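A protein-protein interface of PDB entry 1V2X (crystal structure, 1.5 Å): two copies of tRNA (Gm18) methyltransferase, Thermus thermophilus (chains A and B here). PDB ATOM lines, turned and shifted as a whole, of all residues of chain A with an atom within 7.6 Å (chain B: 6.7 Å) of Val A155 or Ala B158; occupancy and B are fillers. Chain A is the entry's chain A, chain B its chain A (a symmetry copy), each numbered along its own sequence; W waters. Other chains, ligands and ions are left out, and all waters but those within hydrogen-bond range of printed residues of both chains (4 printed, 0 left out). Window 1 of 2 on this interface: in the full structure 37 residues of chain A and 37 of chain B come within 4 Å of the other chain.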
ATOM      1  N   ASN A  35     -19.469 -16.032  -6.545  1.00  0.00           N
ATOM      2  CA  ASN A  35     -18.261 -15.828  -7.369  1.00  0.00           C
ATOM      3  C   ASN A  35     -17.306 -16.989  -7.161  1.00  0.00           C
ATOM      4  O   ASN A  35     -16.706 -17.502  -8.120  1.00  0.00           O
ATOM      5  CB  ASN A  35     -17.598 -14.516  -6.991  1.00  0.00           C
ATOM      6  CG  ASN A  35     -18.357 -13.310  -7.517  1.00  0.00           C
ATOM      7  OD1 ASN A  35     -18.396 -12.251  -6.864  1.00  0.00           O
ATOM      8  ND2 ASN A  35     -18.938 -13.448  -8.704  1.00  0.00           N
ATOM      9  N   ALA A  38     -18.823 -19.967  -9.010  1.00  0.00           N
ATOM     10  CA  ALA A  38     -18.713 -19.845 -10.482  1.00  0.00           C
ATOM     11  C   ALA A  38     -17.274 -19.958 -10.976  1.00  0.00           C
ATOM     12  O   ALA A  38     -17.045 -20.502 -12.069  1.00  0.00           O
ATOM     13  CB  ALA A  38     -19.325 -18.497 -10.988  1.00  0.00           C
ATOM     14  N   ILE A  39     -16.326 -19.447 -10.201  1.00  0.00           N
ATOM     15  CA  ILE A  39     -14.910 -19.509 -10.623  1.00  0.00           C
ATOM     16  C   ILE A  39     -14.403 -20.968 -10.569  1.00  0.00           C
ATOM     17  O   ILE A  39     -13.683 -21.453 -11.466  1.00  0.00           O
ATOM     18  CB  ILE A  39     -14.043 -18.599  -9.765  1.00  0.00           C
ATOM     19  CG1 ILE A  39     -14.409 -17.149 -10.034  1.00  0.00           C
ATOM     20  CG2 ILE A  39     -12.539 -18.900 -10.025  1.00  0.00           C
ATOM     21  CD1 ILE A  39     -13.825 -16.219  -8.980  1.00  0.00           C
ATOM     22  N   THR A  42     -15.706 -22.706 -13.594  1.00  0.00           N
ATOM     23  CA  THR A  42     -14.879 -22.296 -14.743  1.00  0.00           C
ATOM     24  C   THR A  42     -13.543 -23.057 -14.681  1.00  0.00           C
ATOM     25  O   THR A  42     -13.018 -23.547 -15.719  1.00  0.00           O
ATOM     26  CB  THR A  42     -14.637 -20.768 -14.704  1.00  0.00           C
ATOM     27  OG1 THR A  42     -15.890 -20.087 -14.919  1.00  0.00           O
ATOM     28  CG2 THR A  42     -13.640 -20.341 -15.812  1.00  0.00           C
ATOM     29  N   ARG A 109      -4.203 -11.135 -23.452  1.00  0.00           N
ATOM     30  CA  ARG A 109      -4.024 -12.032 -24.581  1.00  0.00           C
ATOM     31  C   ARG A 109      -2.560 -12.152 -25.028  1.00  0.00           C
ATOM     32  O   ARG A 109      -2.217 -13.026 -25.838  1.00  0.00           O
ATOM     33  CB  ARG A 109      -4.903 -11.570 -25.754  1.00  0.00           C
ATOM     34  CG  ARG A 109      -6.419 -11.557 -25.440  1.00  0.00           C
ATOM     35  CD  ARG A 109      -7.214 -10.819 -26.546  1.00  0.00           C
ATOM     36  NE  ARG A 109      -8.660 -10.970 -26.390  1.00  0.00           N
ATOM     37  CZ  ARG A 109      -9.516  -9.978 -26.123  1.00  0.00           C
ATOM     38  NH1 ARG A 109      -9.099  -8.737 -25.987  1.00  0.00           N
ATOM     39  NH2 ARG A 109     -10.805 -10.241 -25.968  1.00  0.00           N
ATOM     40  N   PHE A 121      -6.679 -13.038  -8.638  1.00  0.00           N
ATOM     41  CA  PHE A 121      -7.884 -12.176  -8.787  1.00  0.00           C
ATOM     42  C   PHE A 121      -8.185 -11.590  -7.409  1.00  0.00           C
ATOM     43  O   PHE A 121      -7.928 -12.253  -6.405  1.00  0.00           O
ATOM     44  CB  PHE A 121      -9.069 -13.014  -9.273  1.00  0.00           C
ATOM     45  CG  PHE A 121      -8.857 -13.597 -10.635  1.00  0.00           C
ATOM     46  CD1 PHE A 121      -8.224 -14.832 -10.790  1.00  0.00           C
ATOM     47  CD2 PHE A 121      -9.282 -12.888 -11.758  1.00  0.00           C
ATOM     48  CE1 PHE A 121      -8.004 -15.367 -12.071  1.00  0.00           C
ATOM     49  CE2 PHE A 121      -9.074 -13.400 -13.048  1.00  0.00           C
ATOM     50  CZ  PHE A 121      -8.428 -14.648 -13.205  1.00  0.00           C
ATOM     51  N   ILE A 142      -7.841  -7.000 -18.866  1.00  0.00           N
ATOM     52  CA  ILE A 142      -8.747  -7.362 -19.954  1.00  0.00           C
ATOM     53  C   ILE A 142      -9.266  -6.007 -20.502  1.00  0.00           C
ATOM     54  O   ILE A 142      -9.756  -5.193 -19.749  1.00  0.00           O
ATOM     55  CB  ILE A 142      -9.961  -8.219 -19.450  1.00  0.00           C
ATOM     56  CG1 ILE A 142      -9.480  -9.606 -19.006  1.00  0.00           C
ATOM     57  CG2 ILE A 142     -10.979  -8.413 -20.578  1.00  0.00           C
ATOM     58  CD1 ILE A 142     -10.509 -10.348 -18.160  1.00  0.00           C
ATOM     59  N   MET A 144     -11.318  -2.930 -21.628  1.00  0.00           N
ATOM     60  CA  MET A 144     -12.676  -2.502 -21.296  1.00  0.00           C
ATOM     61  C   MET A 144     -12.963  -1.375 -22.280  1.00  0.00           C
ATOM     62  O   MET A 144     -12.347  -0.315 -22.190  1.00  0.00           O
ATOM     63  CB  MET A 144     -12.723  -1.973 -19.868  1.00  0.00           C
ATOM     64  CG  MET A 144     -12.297  -2.991 -18.778  1.00  0.00           C
ATOM     65  SD  MET A 144     -13.484  -4.296 -18.590  1.00  0.00           S
ATOM     66  CE  MET A 144     -12.719  -5.522 -19.540  1.00  0.00           C
ATOM     67  N   LEU A 151     -14.915  -5.582 -14.694  1.00  0.00           N
ATOM     68  CA  LEU A 151     -15.849  -6.679 -14.920  1.00  0.00           C
ATOM     69  C   LEU A 151     -16.114  -7.383 -13.579  1.00  0.00           C
ATOM     70  O   LEU A 151     -15.386  -7.185 -12.590  1.00  0.00           O
ATOM     71  CB  LEU A 151     -15.231  -7.737 -15.837  1.00  0.00           C
ATOM     72  CG  LEU A 151     -14.915  -7.340 -17.273  1.00  0.00           C
ATOM     73  CD1 LEU A 151     -13.939  -8.365 -17.843  1.00  0.00           C
ATOM     74  CD2 LEU A 151     -16.253  -7.271 -18.096  1.00  0.00           C
ATOM     75  N   ASN A 152     -17.161  -8.198 -13.559  1.00  0.00           N
ATOM     76  CA  ASN A 152     -17.462  -9.015 -12.364  1.00  0.00           C
ATOM     77  C   ASN A 152     -16.205  -9.939 -12.218  1.00  0.00           C
ATOM     78  O   ASN A 152     -15.628 -10.344 -13.221  1.00  0.00           O
ATOM     79  CB  ASN A 152     -18.706  -9.863 -12.608  1.00  0.00           C
ATOM     80  CG  ASN A 152     -18.756 -11.063 -11.687  1.00  0.00           C
ATOM     81  OD1 ASN A 152     -19.238 -10.978 -10.553  1.00  0.00           O
ATOM     82  ND2 ASN A 152     -18.214 -12.178 -12.152  1.00  0.00           N
ATOM     83  N   VAL A 153     -15.763 -10.252 -11.008  1.00  0.00           N
ATOM     84  CA  VAL A 153     -14.515 -11.049 -10.864  1.00  0.00           C
ATOM     85  C   VAL A 153     -14.576 -12.448 -11.491  1.00  0.00           C
ATOM     86  O   VAL A 153     -13.582 -12.930 -12.094  1.00  0.00           O
ATOM     87  CB  VAL A 153     -14.064 -11.118  -9.349  1.00  0.00           C
ATOM     88  CG1 VAL A 153     -15.105 -11.804  -8.466  1.00  0.00           C
ATOM     89  CG2 VAL A 153     -12.760 -11.872  -9.215  1.00  0.00           C
ATOM     90  N   SER A 154     -15.719 -13.117 -11.361  1.00  0.00           N
ATOM     91  CA  SER A 154     -15.912 -14.446 -11.931  1.00  0.00           C
ATOM     92  C   SER A 154     -15.852 -14.316 -13.445  1.00  0.00           C
ATOM     93  O   SER A 154     -15.309 -15.169 -14.155  1.00  0.00           O
ATOM     94  CB  SER A 154     -17.275 -15.014 -11.530  1.00  0.00           C
ATOM     95  OG  SER A 154     -17.529 -16.228 -12.238  1.00  0.00           O
ATOM     96  N   VAL A 155     -16.439 -13.235 -13.963  1.00  0.00           N
ATOM     97  CA  VAL A 155     -16.378 -13.034 -15.382  1.00  0.00           C
ATOM     98  C   VAL A 155     -14.947 -12.823 -15.833  1.00  0.00           C
ATOM     99  O   VAL A 155     -14.527 -13.384 -16.876  1.00  0.00           O
ATOM    100  CB  VAL A 155     -17.213 -11.824 -15.788  1.00  0.00           C
ATOM    101  CG1 VAL A 155     -16.789 -11.351 -17.136  1.00  0.00           C
ATOM    102  CG2 VAL A 155     -18.699 -12.228 -15.780  1.00  0.00           C
ATOM    103  N   ALA A 156     -14.191 -12.003 -15.097  1.00  0.00           N
ATOM    104  CA  ALA A 156     -12.807 -11.750 -15.500  1.00  0.00           C
ATOM    105  C   ALA A 156     -12.042 -13.061 -15.466  1.00  0.00           C
ATOM    106  O   ALA A 156     -11.220 -13.348 -16.341  1.00  0.00           O
ATOM    107  CB  ALA A 156     -12.133 -10.729 -14.583  1.00  0.00           C
ATOM    108  N   ALA A 157     -12.256 -13.850 -14.428  1.00  0.00           N
ATOM    109  CA  ALA A 157     -11.538 -15.139 -14.339  1.00  0.00           C
ATOM    110  C   ALA A 157     -11.802 -16.044 -15.553  1.00  0.00           C
ATOM    111  O   ALA A 157     -10.892 -16.751 -16.027  1.00  0.00           O
ATOM    112  CB  ALA A 157     -11.948 -15.880 -13.060  1.00  0.00           C
ATOM    113  N   ALA A 158     -13.046 -16.062 -16.025  1.00  0.00           N
ATOM    114  CA  ALA A 158     -13.435 -16.909 -17.158  1.00  0.00           C
ATOM    115  C   ALA A 158     -12.817 -16.404 -18.466  1.00  0.00           C
ATOM    116  O   ALA A 158     -12.371 -17.199 -19.301  1.00  0.00           O
ATOM    117  CB  ALA A 158     -14.953 -16.919 -17.271  1.00  0.00           C
ATOM    118  N   VAL A 159     -12.840 -15.089 -18.667  1.00  0.00           N
ATOM    119  CA  VAL A 159     -12.241 -14.511 -19.907  1.00  0.00           C
ATOM    120  C   VAL A 159     -10.773 -14.903 -19.994  1.00  0.00           C
ATOM    121  O   VAL A 159     -10.297 -15.369 -21.032  1.00  0.00           O
ATOM    122  CB  VAL A 159     -12.431 -12.968 -19.912  1.00  0.00           C
ATOM    123  CG1 VAL A 159     -11.627 -12.280 -21.040  1.00  0.00           C
ATOM    124  CG2 VAL A 159     -13.898 -12.655 -20.075  1.00  0.00           C
ATOM    125  N   ILE A 160     -10.043 -14.750 -18.911  1.00  0.00           N
ATOM    126  CA  ILE A 160      -8.637 -15.146 -18.902  1.00  0.00           C
ATOM    127  C   ILE A 160      -8.447 -16.687 -18.976  1.00  0.00           C
ATOM    128  O   ILE A 160      -7.652 -17.202 -19.769  1.00  0.00           O
ATOM    129  CB  ILE A 160      -7.947 -14.563 -17.633  1.00  0.00           C
ATOM    130  CG1 ILE A 160      -7.850 -13.038 -17.762  1.00  0.00           C
ATOM    131  CG2 ILE A 160      -6.535 -15.139 -17.462  1.00  0.00           C
ATOM    132  CD1 ILE A 160      -7.626 -12.316 -16.474  1.00  0.00           C
ATOM    133  N   LEU A 161      -9.161 -17.461 -18.161  1.00  0.00           N
ATOM    134  CA  LEU A 161      -8.967 -18.911 -18.210  1.00  0.00           C
ATOM    135  C   LEU A 161      -9.390 -19.536 -19.561  1.00  0.00           C
ATOM    136  O   LEU A 161      -8.811 -20.548 -19.985  1.00  0.00           O
ATOM    137  CB  LEU A 161      -9.726 -19.573 -17.048  1.00  0.00           C
ATOM    138  CG  LEU A 161      -9.036 -19.417 -15.688  1.00  0.00           C
ATOM    139  CD1 LEU A 161     -10.001 -19.915 -14.644  1.00  0.00           C
ATOM    140  CD2 LEU A 161      -7.743 -20.211 -15.626  1.00  0.00           C
ATOM    141  N   PHE A 162     -10.387 -18.951 -20.254  1.00  0.00           N
ATOM    142  CA  PHE A 162     -10.760 -19.557 -21.540  1.00  0.00           C
ATOM    143  C   PHE A 162      -9.777 -19.136 -22.635  1.00  0.00           C
ATOM    144  O   PHE A 162      -9.720 -19.810 -23.657  1.00  0.00           O
ATOM    145  CB  PHE A 162     -12.228 -19.324 -21.917  1.00  0.00           C
ATOM    146  CG  PHE A 162     -13.181 -20.366 -21.310  1.00  0.00           C
ATOM    147  CD1 PHE A 162     -13.716 -20.193 -20.030  1.00  0.00           C
ATOM    148  CD2 PHE A 162     -13.481 -21.525 -21.991  1.00  0.00           C
ATOM    149  CE1 PHE A 162     -14.526 -21.168 -19.466  1.00  0.00           C
ATOM    150  CE2 PHE A 162     -14.298 -22.521 -21.443  1.00  0.00           C
ATOM    151  CZ  PHE A 162     -14.823 -22.335 -20.169  1.00  0.00           C
ATOM    152  N   ALA B  38     -24.343  -8.742 -14.139  1.00  0.00           N
ATOM    153  CA  ALA B  38     -22.990  -9.054 -14.657  1.00  0.00           C
ATOM    154  C   ALA B  38     -22.947  -9.133 -16.180  1.00  0.00           C
ATOM    155  O   ALA B  38     -21.930  -8.751 -16.782  1.00  0.00           O
ATOM    156  CB  ALA B  38     -22.448 -10.392 -14.057  1.00  0.00           C
ATOM    157  N   ILE B  39     -24.016  -9.629 -16.791  1.00  0.00           N
ATOM    158  CA  ILE B  39     -24.038  -9.748 -18.265  1.00  0.00           C
ATOM    159  C   ILE B  39     -24.110  -8.345 -18.909  1.00  0.00           C
ATOM    160  O   ILE B  39     -23.433  -8.041 -19.914  1.00  0.00           O
ATOM    161  CB  ILE B  39     -25.197 -10.619 -18.726  1.00  0.00           C
ATOM    162  CG1 ILE B  39     -24.962 -12.053 -18.278  1.00  0.00           C
ATOM    163  CG2 ILE B  39     -25.378 -10.491 -20.265  1.00  0.00           C
ATOM    164  CD1 ILE B  39     -26.223 -12.894 -18.410  1.00  0.00           C
ATOM    165  N   THR B  42     -20.688  -6.882 -18.767  1.00  0.00           N
ATOM    166  CA  THR B  42     -19.885  -7.504 -19.835  1.00  0.00           C
ATOM    167  C   THR B  42     -20.280  -6.865 -21.178  1.00  0.00           C
ATOM    168  O   THR B  42     -19.409  -6.556 -22.039  1.00  0.00           O
ATOM    169  CB  THR B  42     -20.134  -9.031 -19.865  1.00  0.00           C
ATOM    170  OG1 THR B  42     -19.613  -9.617 -18.655  1.00  0.00           O
ATOM    171  CG2 THR B  42     -19.423  -9.679 -21.081  1.00  0.00           C
ATOM    172  N   VAL B  46     -17.644  -4.765 -23.937  1.00  0.00           N
ATOM    173  CA  VAL B  46     -17.340  -5.132 -25.340  1.00  0.00           C
ATOM    174  C   VAL B  46     -18.022  -4.202 -26.334  1.00  0.00           C
ATOM    175  O   VAL B  46     -17.974  -4.428 -27.547  1.00  0.00           O
ATOM    176  CB  VAL B  46     -17.703  -6.607 -25.655  1.00  0.00           C
ATOM    177  CG1 VAL B  46     -16.964  -7.509 -24.711  1.00  0.00           C
ATOM    178  CG2 VAL B  46     -19.217  -6.877 -25.610  1.00  0.00           C
ATOM    179  N   THR B  66     -23.371  -6.984  -9.841  1.00  0.00           N
ATOM    180  CA  THR B  66     -22.498  -6.124 -10.617  1.00  0.00           C
ATOM    181  C   THR B  66     -23.320  -4.967 -11.098  1.00  0.00           C
ATOM    182  O   THR B  66     -24.489  -4.807 -10.751  1.00  0.00           O
ATOM    183  CB  THR B  66     -21.923  -6.736 -11.895  1.00  0.00           C
ATOM    184  OG1 THR B  66     -22.991  -6.992 -12.800  1.00  0.00           O
ATOM    185  CG2 THR B  66     -21.146  -7.990 -11.623  1.00  0.00           C
ATOM    186  N   PHE B 121     -28.997 -16.643 -24.700  1.00  0.00           N
ATOM    187  CA  PHE B 121     -28.570 -17.405 -23.494  1.00  0.00           C
ATOM    188  C   PHE B 121     -29.840 -17.786 -22.735  1.00  0.00           C
ATOM    189  O   PHE B 121     -30.810 -17.031 -22.768  1.00  0.00           O
ATOM    190  CB  PHE B 121     -27.674 -16.529 -22.614  1.00  0.00           C
ATOM    191  CG  PHE B 121     -26.393 -16.140 -23.283  1.00  0.00           C
ATOM    192  CD1 PHE B 121     -26.326 -14.996 -24.081  1.00  0.00           C
ATOM    193  CD2 PHE B 121     -25.263 -16.940 -23.119  1.00  0.00           C
ATOM    194  CE1 PHE B 121     -25.128 -14.645 -24.727  1.00  0.00           C
ATOM    195  CE2 PHE B 121     -24.056 -16.613 -23.754  1.00  0.00           C
ATOM    196  CZ  PHE B 121     -23.990 -15.456 -24.566  1.00  0.00           C
ATOM    197  N   ILE B 142     -19.489 -23.765 -25.827  1.00  0.00           N
ATOM    198  CA  ILE B 142     -18.149 -23.460 -25.328  1.00  0.00           C
ATOM    199  C   ILE B 142     -17.595 -24.819 -24.829  1.00  0.00           C
ATOM    200  O   ILE B 142     -18.235 -25.486 -24.044  1.00  0.00           O
ATOM    201  CB  ILE B 142     -18.182 -22.441 -24.136  1.00  0.00           C
ATOM    202  CG1 ILE B 142     -18.624 -21.059 -24.634  1.00  0.00           C
ATOM    203  CG2 ILE B 142     -16.786 -22.296 -23.522  1.00  0.00           C
ATOM    204  CD1 ILE B 142     -19.048 -20.129 -23.503  1.00  0.00           C
ATOM    205  N   ASN B 152     -21.596 -21.084 -15.589  1.00  0.00           N
ATOM    206  CA  ASN B 152     -22.565 -20.102 -15.057  1.00  0.00           C
ATOM    207  C   ASN B 152     -23.000 -19.285 -16.321  1.00  0.00           C
ATOM    208  O   ASN B 152     -22.186 -19.060 -17.209  1.00  0.00           O
ATOM    209  CB  ASN B 152     -21.880 -19.180 -14.051  1.00  0.00           C
ATOM    210  CG  ASN B 152     -22.630 -17.877 -13.884  1.00  0.00           C
ATOM    211  OD1 ASN B 152     -23.567 -17.778 -13.086  1.00  0.00           O
ATOM    212  ND2 ASN B 152     -22.252 -16.881 -14.671  1.00  0.00           N
ATOM    213  N   VAL B 153     -24.253 -18.866 -16.427  1.00  0.00           N
ATOM    214  CA  VAL B 153     -24.695 -18.174 -17.667  1.00  0.00           C
ATOM    215  C   VAL B 153     -23.955 -16.862 -17.964  1.00  0.00           C
ATOM    216  O   VAL B 153     -23.640 -16.551 -19.141  1.00  0.00           O
ATOM    217  CB  VAL B 153     -26.262 -17.959 -17.663  1.00  0.00           C
ATOM    218  CG1 VAL B 153     -26.724 -17.079 -16.503  1.00  0.00           C
ATOM    219  CG2 VAL B 153     -26.716 -17.316 -18.954  1.00  0.00           C
ATOM    220  N   SER B 154     -23.671 -16.082 -16.924  1.00  0.00           N
ATOM    221  CA  SER B 154     -22.952 -14.822 -17.070  1.00  0.00           C
ATOM    222  C   SER B 154     -21.546 -15.142 -17.551  1.00  0.00           C
ATOM    223  O   SER B 154     -20.959 -14.435 -18.378  1.00  0.00           O
ATOM    224  CB  SER B 154     -22.869 -14.087 -15.730  1.00  0.00           C
ATOM    225  OG  SER B 154     -22.011 -12.952 -15.845  1.00  0.00           O
ATOM    226  N   VAL B 155     -20.975 -16.221 -17.012  1.00  0.00           N
ATOM    227  CA  VAL B 155     -19.664 -16.600 -17.458  1.00  0.00           C
ATOM    228  C   VAL B 155     -19.688 -16.993 -18.920  1.00  0.00           C
ATOM    229  O   VAL B 155     -18.775 -16.606 -19.691  1.00  0.00           O
ATOM    230  CB  VAL B 155     -19.137 -17.770 -16.634  1.00  0.00           C
ATOM    231  CG1 VAL B 155     -18.029 -18.442 -17.371  1.00  0.00           C
ATOM    232  CG2 VAL B 155     -18.658 -17.236 -15.272  1.00  0.00           C
ATOM    233  N   ALA B 156     -20.691 -17.781 -19.323  1.00  0.00           N
ATOM    234  CA  ALA B 156     -20.749 -18.206 -20.722  1.00  0.00           C
ATOM    235  C   ALA B 156     -20.894 -16.976 -21.599  1.00  0.00           C
ATOM    236  O   ALA B 156     -20.287 -16.875 -22.669  1.00  0.00           O
ATOM    237  CB  ALA B 156     -21.915 -19.164 -20.969  1.00  0.00           C
ATOM    238  N   ALA B 157     -21.743 -16.050 -21.192  1.00  0.00           N
ATOM    239  CA  ALA B 157     -21.928 -14.830 -22.006  1.00  0.00           C
ATOM    240  C   ALA B 157     -20.614 -14.061 -22.221  1.00  0.00           C
ATOM    241  O   ALA B 157     -20.376 -13.503 -23.308  1.00  0.00           O
ATOM    242  CB  ALA B 157     -22.950 -13.902 -21.337  1.00  0.00           C
ATOM    243  N   ALA B 158     -19.789 -13.988 -21.179  1.00  0.00           N
ATOM    244  CA  ALA B 158     -18.519 -13.256 -21.244  1.00  0.00           C
ATOM    245  C   ALA B 158     -17.510 -13.972 -22.148  1.00  0.00           C
ATOM    246  O   ALA B 158     -16.781 -13.330 -22.913  1.00  0.00           O
ATOM    247  CB  ALA B 158     -17.951 -13.122 -19.838  1.00  0.00           C
ATOM    248  N   VAL B 159     -17.432 -15.294 -22.023  1.00  0.00           N
ATOM    249  CA  VAL B 159     -16.490 -16.072 -22.881  1.00  0.00           C
ATOM    250  C   VAL B 159     -16.816 -15.829 -24.347  1.00  0.00           C
ATOM    251  O   VAL B 159     -15.932 -15.540 -25.158  1.00  0.00           O
ATOM    252  CB  VAL B 159     -16.567 -17.581 -22.512  1.00  0.00           C
ATOM    253  CG1 VAL B 159     -15.802 -18.473 -23.518  1.00  0.00           C
ATOM    254  CG2 VAL B 159     -15.996 -17.777 -21.129  1.00  0.00           C
ATOM    255  N   ILE B 160     -18.077 -15.912 -24.707  1.00  0.00           N
ATOM    256  CA  ILE B 160     -18.476 -15.648 -26.087  1.00  0.00           C
ATOM    257  C   ILE B 160     -18.323 -14.151 -26.478  1.00  0.00           C
ATOM    258  O   ILE B 160     -17.765 -13.812 -27.527  1.00  0.00           O
ATOM    259  CB  ILE B 160     -19.941 -16.130 -26.300  1.00  0.00           C
ATOM    260  CG1 ILE B 160     -19.987 -17.662 -26.242  1.00  0.00           C
ATOM    261  CG2 ILE B 160     -20.479 -15.668 -27.661  1.00  0.00           C
ATOM    262  CD1 ILE B 160     -21.341 -18.237 -25.991  1.00  0.00           C
ATOM    263  N   LEU B 161     -18.810 -13.221 -25.659  1.00  0.00           N
ATOM    264  CA  LEU B 161     -18.691 -11.812 -26.036  1.00  0.00           C
ATOM    265  C   LEU B 161     -17.225 -11.322 -26.104  1.00  0.00           C
ATOM    266  O   LEU B 161     -16.906 -10.427 -26.902  1.00  0.00           O
ATOM    267  CB  LEU B 161     -19.504 -10.946 -25.060  1.00  0.00           C
ATOM    268  CG  LEU B 161     -21.017 -10.995 -25.299  1.00  0.00           C
ATOM    269  CD1 LEU B 161     -21.671 -10.287 -24.141  1.00  0.00           C
ATOM    270  CD2 LEU B 161     -21.395 -10.319 -26.606  1.00  0.00           C
ATOM    271  N   PHE B 162     -16.318 -11.896 -25.288  1.00  0.00           N
ATOM    272  CA  PHE B 162     -14.931 -11.421 -25.383  1.00  0.00           C
ATOM    273  C   PHE B 162     -14.227 -12.061 -26.582  1.00  0.00           C
ATOM    274  O   PHE B 162     -13.213 -11.526 -27.016  1.00  0.00           O
ATOM    275  CB  PHE B 162     -14.150 -11.565 -24.071  1.00  0.00           C
ATOM    276  CG  PHE B 162     -14.343 -10.374 -23.118  1.00  0.00           C
ATOM    277  CD1 PHE B 162     -15.411 -10.339 -22.217  1.00  0.00           C
ATOM    278  CD2 PHE B 162     -13.501  -9.286 -23.174  1.00  0.00           C
ATOM    279  CE1 PHE B 162     -15.614  -9.232 -21.405  1.00  0.00           C
ATOM    280  CE2 PHE B 162     -13.684  -8.160 -22.363  1.00  0.00           C
ATOM    281  CZ  PHE B 162     -14.751  -8.139 -21.471  1.00  0.00           C
ATOM    282  N   GLU B 163     -14.754 -13.180 -27.109  1.00  0.00           N
ATOM    283  CA  GLU B 163     -14.191 -13.768 -28.355  1.00  0.00           C
ATOM    284  C   GLU B 163     -14.700 -12.776 -29.438  1.00  0.00           C
ATOM    285  O   GLU B 163     -13.970 -12.419 -30.366  1.00  0.00           O
ATOM    286  CB  GLU B 163     -14.700 -15.229 -28.598  1.00  0.00           C
ATOM    287  CG  GLU B 163     -14.416 -15.832 -30.028  1.00  0.00           C
ATOM    288  CD  GLU B 163     -12.975 -15.691 -30.463  1.00  0.00           C
ATOM    289  OE1 GLU B 163     -12.115 -15.477 -29.582  1.00  0.00           O
ATOM    290  OE2 GLU B 163     -12.689 -15.774 -31.691  1.00  0.00           O
ATOM    291  N   ALA B 164     -15.946 -12.297 -29.335  1.00  0.00           N
ATOM    292  CA  ALA B 164     -16.456 -11.308 -30.302  1.00  0.00           C
ATOM    293  C   ALA B 164     -15.621 -10.024 -30.192  1.00  0.00           C
ATOM    294  O   ALA B 164     -15.268  -9.395 -31.216  1.00  0.00           O
ATOM    295  CB  ALA B 164     -17.950 -10.991 -30.024  1.00  0.00           C
HETATM  296  O   HOH W   1     -18.704 -20.893 -14.533  1.00  0.00           O
HETATM  297  O   HOH W   2     -20.248 -15.649 -12.698  1.00  0.00           O
HETATM  298  O   HOH W   3     -20.804 -13.334 -13.328  1.00  0.00           O
HETATM  299  O   HOH W   4     -19.055  -8.518 -15.972  1.00  0.00           O
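Of the 20 printed residues of chain B, 8 touch a printed residue of chain A. Hydrophobic or aromatic side chains of chain B within 4 Å of the printed part of chain A: Ile B142, Val B155, Ala B158, Val B159 and Phe B162. Of the 20 printed residues of chain A, 11 touch a printed residue of chain B. Among the printed residues, 14 pairs touch across the chains. Among the printed residues, no Asp or Glu carboxylate lies within 4 Å of a Lys or Arg side-chain nitrogen of the other chain.
Among the printed residues, merely in contact across the chains: Asn A152 with Thr B66, Phe A162 with Ile B142, Ile A142 with Phe B162, Ser A154 with Val B155, Val A155 with Ser B154, Val A155 with Ala B158, Ala A158 with Val B155, Val A159 with Phe B162, Phe A162 with Val B159, Val A155 with Thr B42, Thr A42 with Val B155, Leu A151 with Phe B162 and Met A144 with Phe B162.
Water W2 bridges OG of Ser A154 and ND2 of Asn B152. Water W3 bridges the side-chain hydroxyl (OG) of Ser B154 (2.8 Å) and the side-chain amide nitrogen (ND2) of Asn A152 (3.1 Å). Water W1 lies within hydrogen-bond range of OG1 of Thr A42 (3.0 Å), O of Ala A38 (3.0 Å) and N of Asn B152 (3.1 Å). Water W4 lies within hydrogen-bond range of OG1 of Thr B42 (3.0 Å), O of Ala B38 (3.0 Å) and N of Asn A152 (3.1 Å).
The backbone carbonyl oxygen (O) of Phe B162 is in hydrogen-bond range of the guanidinium group (NH2) of Arg A109 (2.9 Å).
Printed residues of chain B within 4 Å of Arg A109: Phe B162 (2.9 Å). Of the printed residues of chain B, Leu A151 touches Phe B162. Printed residues of chain A within 4 Å of Ala B158: Val A155. Of the printed residues of chain A, Phe B162 touches Arg A109, Ile A142, Met A144, Leu A151 and Val A159. The nearest printed residue of chain B that does not touch Phe A162 is Val B155 (4.9 Å).
ND2 of Asn A35 lies within hydrogen-bond range of OD1 of Asn A152 (3.1 Å). The side-chain hydroxyl (OG1) of Thr A42 is in hydrogen-bond range of the backbone carbonyl oxygen (O) of Ala A38, at 3.1 Å. The side-chain amide nitrogen (ND2) of Asn A152 sits close to the backbone NH (N) of Ser A154 (2.8 Å). The side-chain amide nitrogen (ND2) of Asn A152 sits close to the backbone NH (N) of Val A155 (2.7 Å). N of Ala B38 sits at hydrogen-bond distance from OG1 of Thr B66 (2.6 Å). N of Ser B154 sits close to ND2 of Asn B152 (2.8 Å).
Thr A42 touches Val B155, and with the chains exchanged Val A155 touches Thr B42. Ser A154 touches Val B155, and with the chains exchanged Val A155 touches Ser B154. Val A155 touches Ala B158, and with the chains exchanged Ala A158 touches Val B155. Val A159 touches Phe B162, and with the chains exchanged Phe A162 touches Val B159. 16 positions are printed for both chains.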
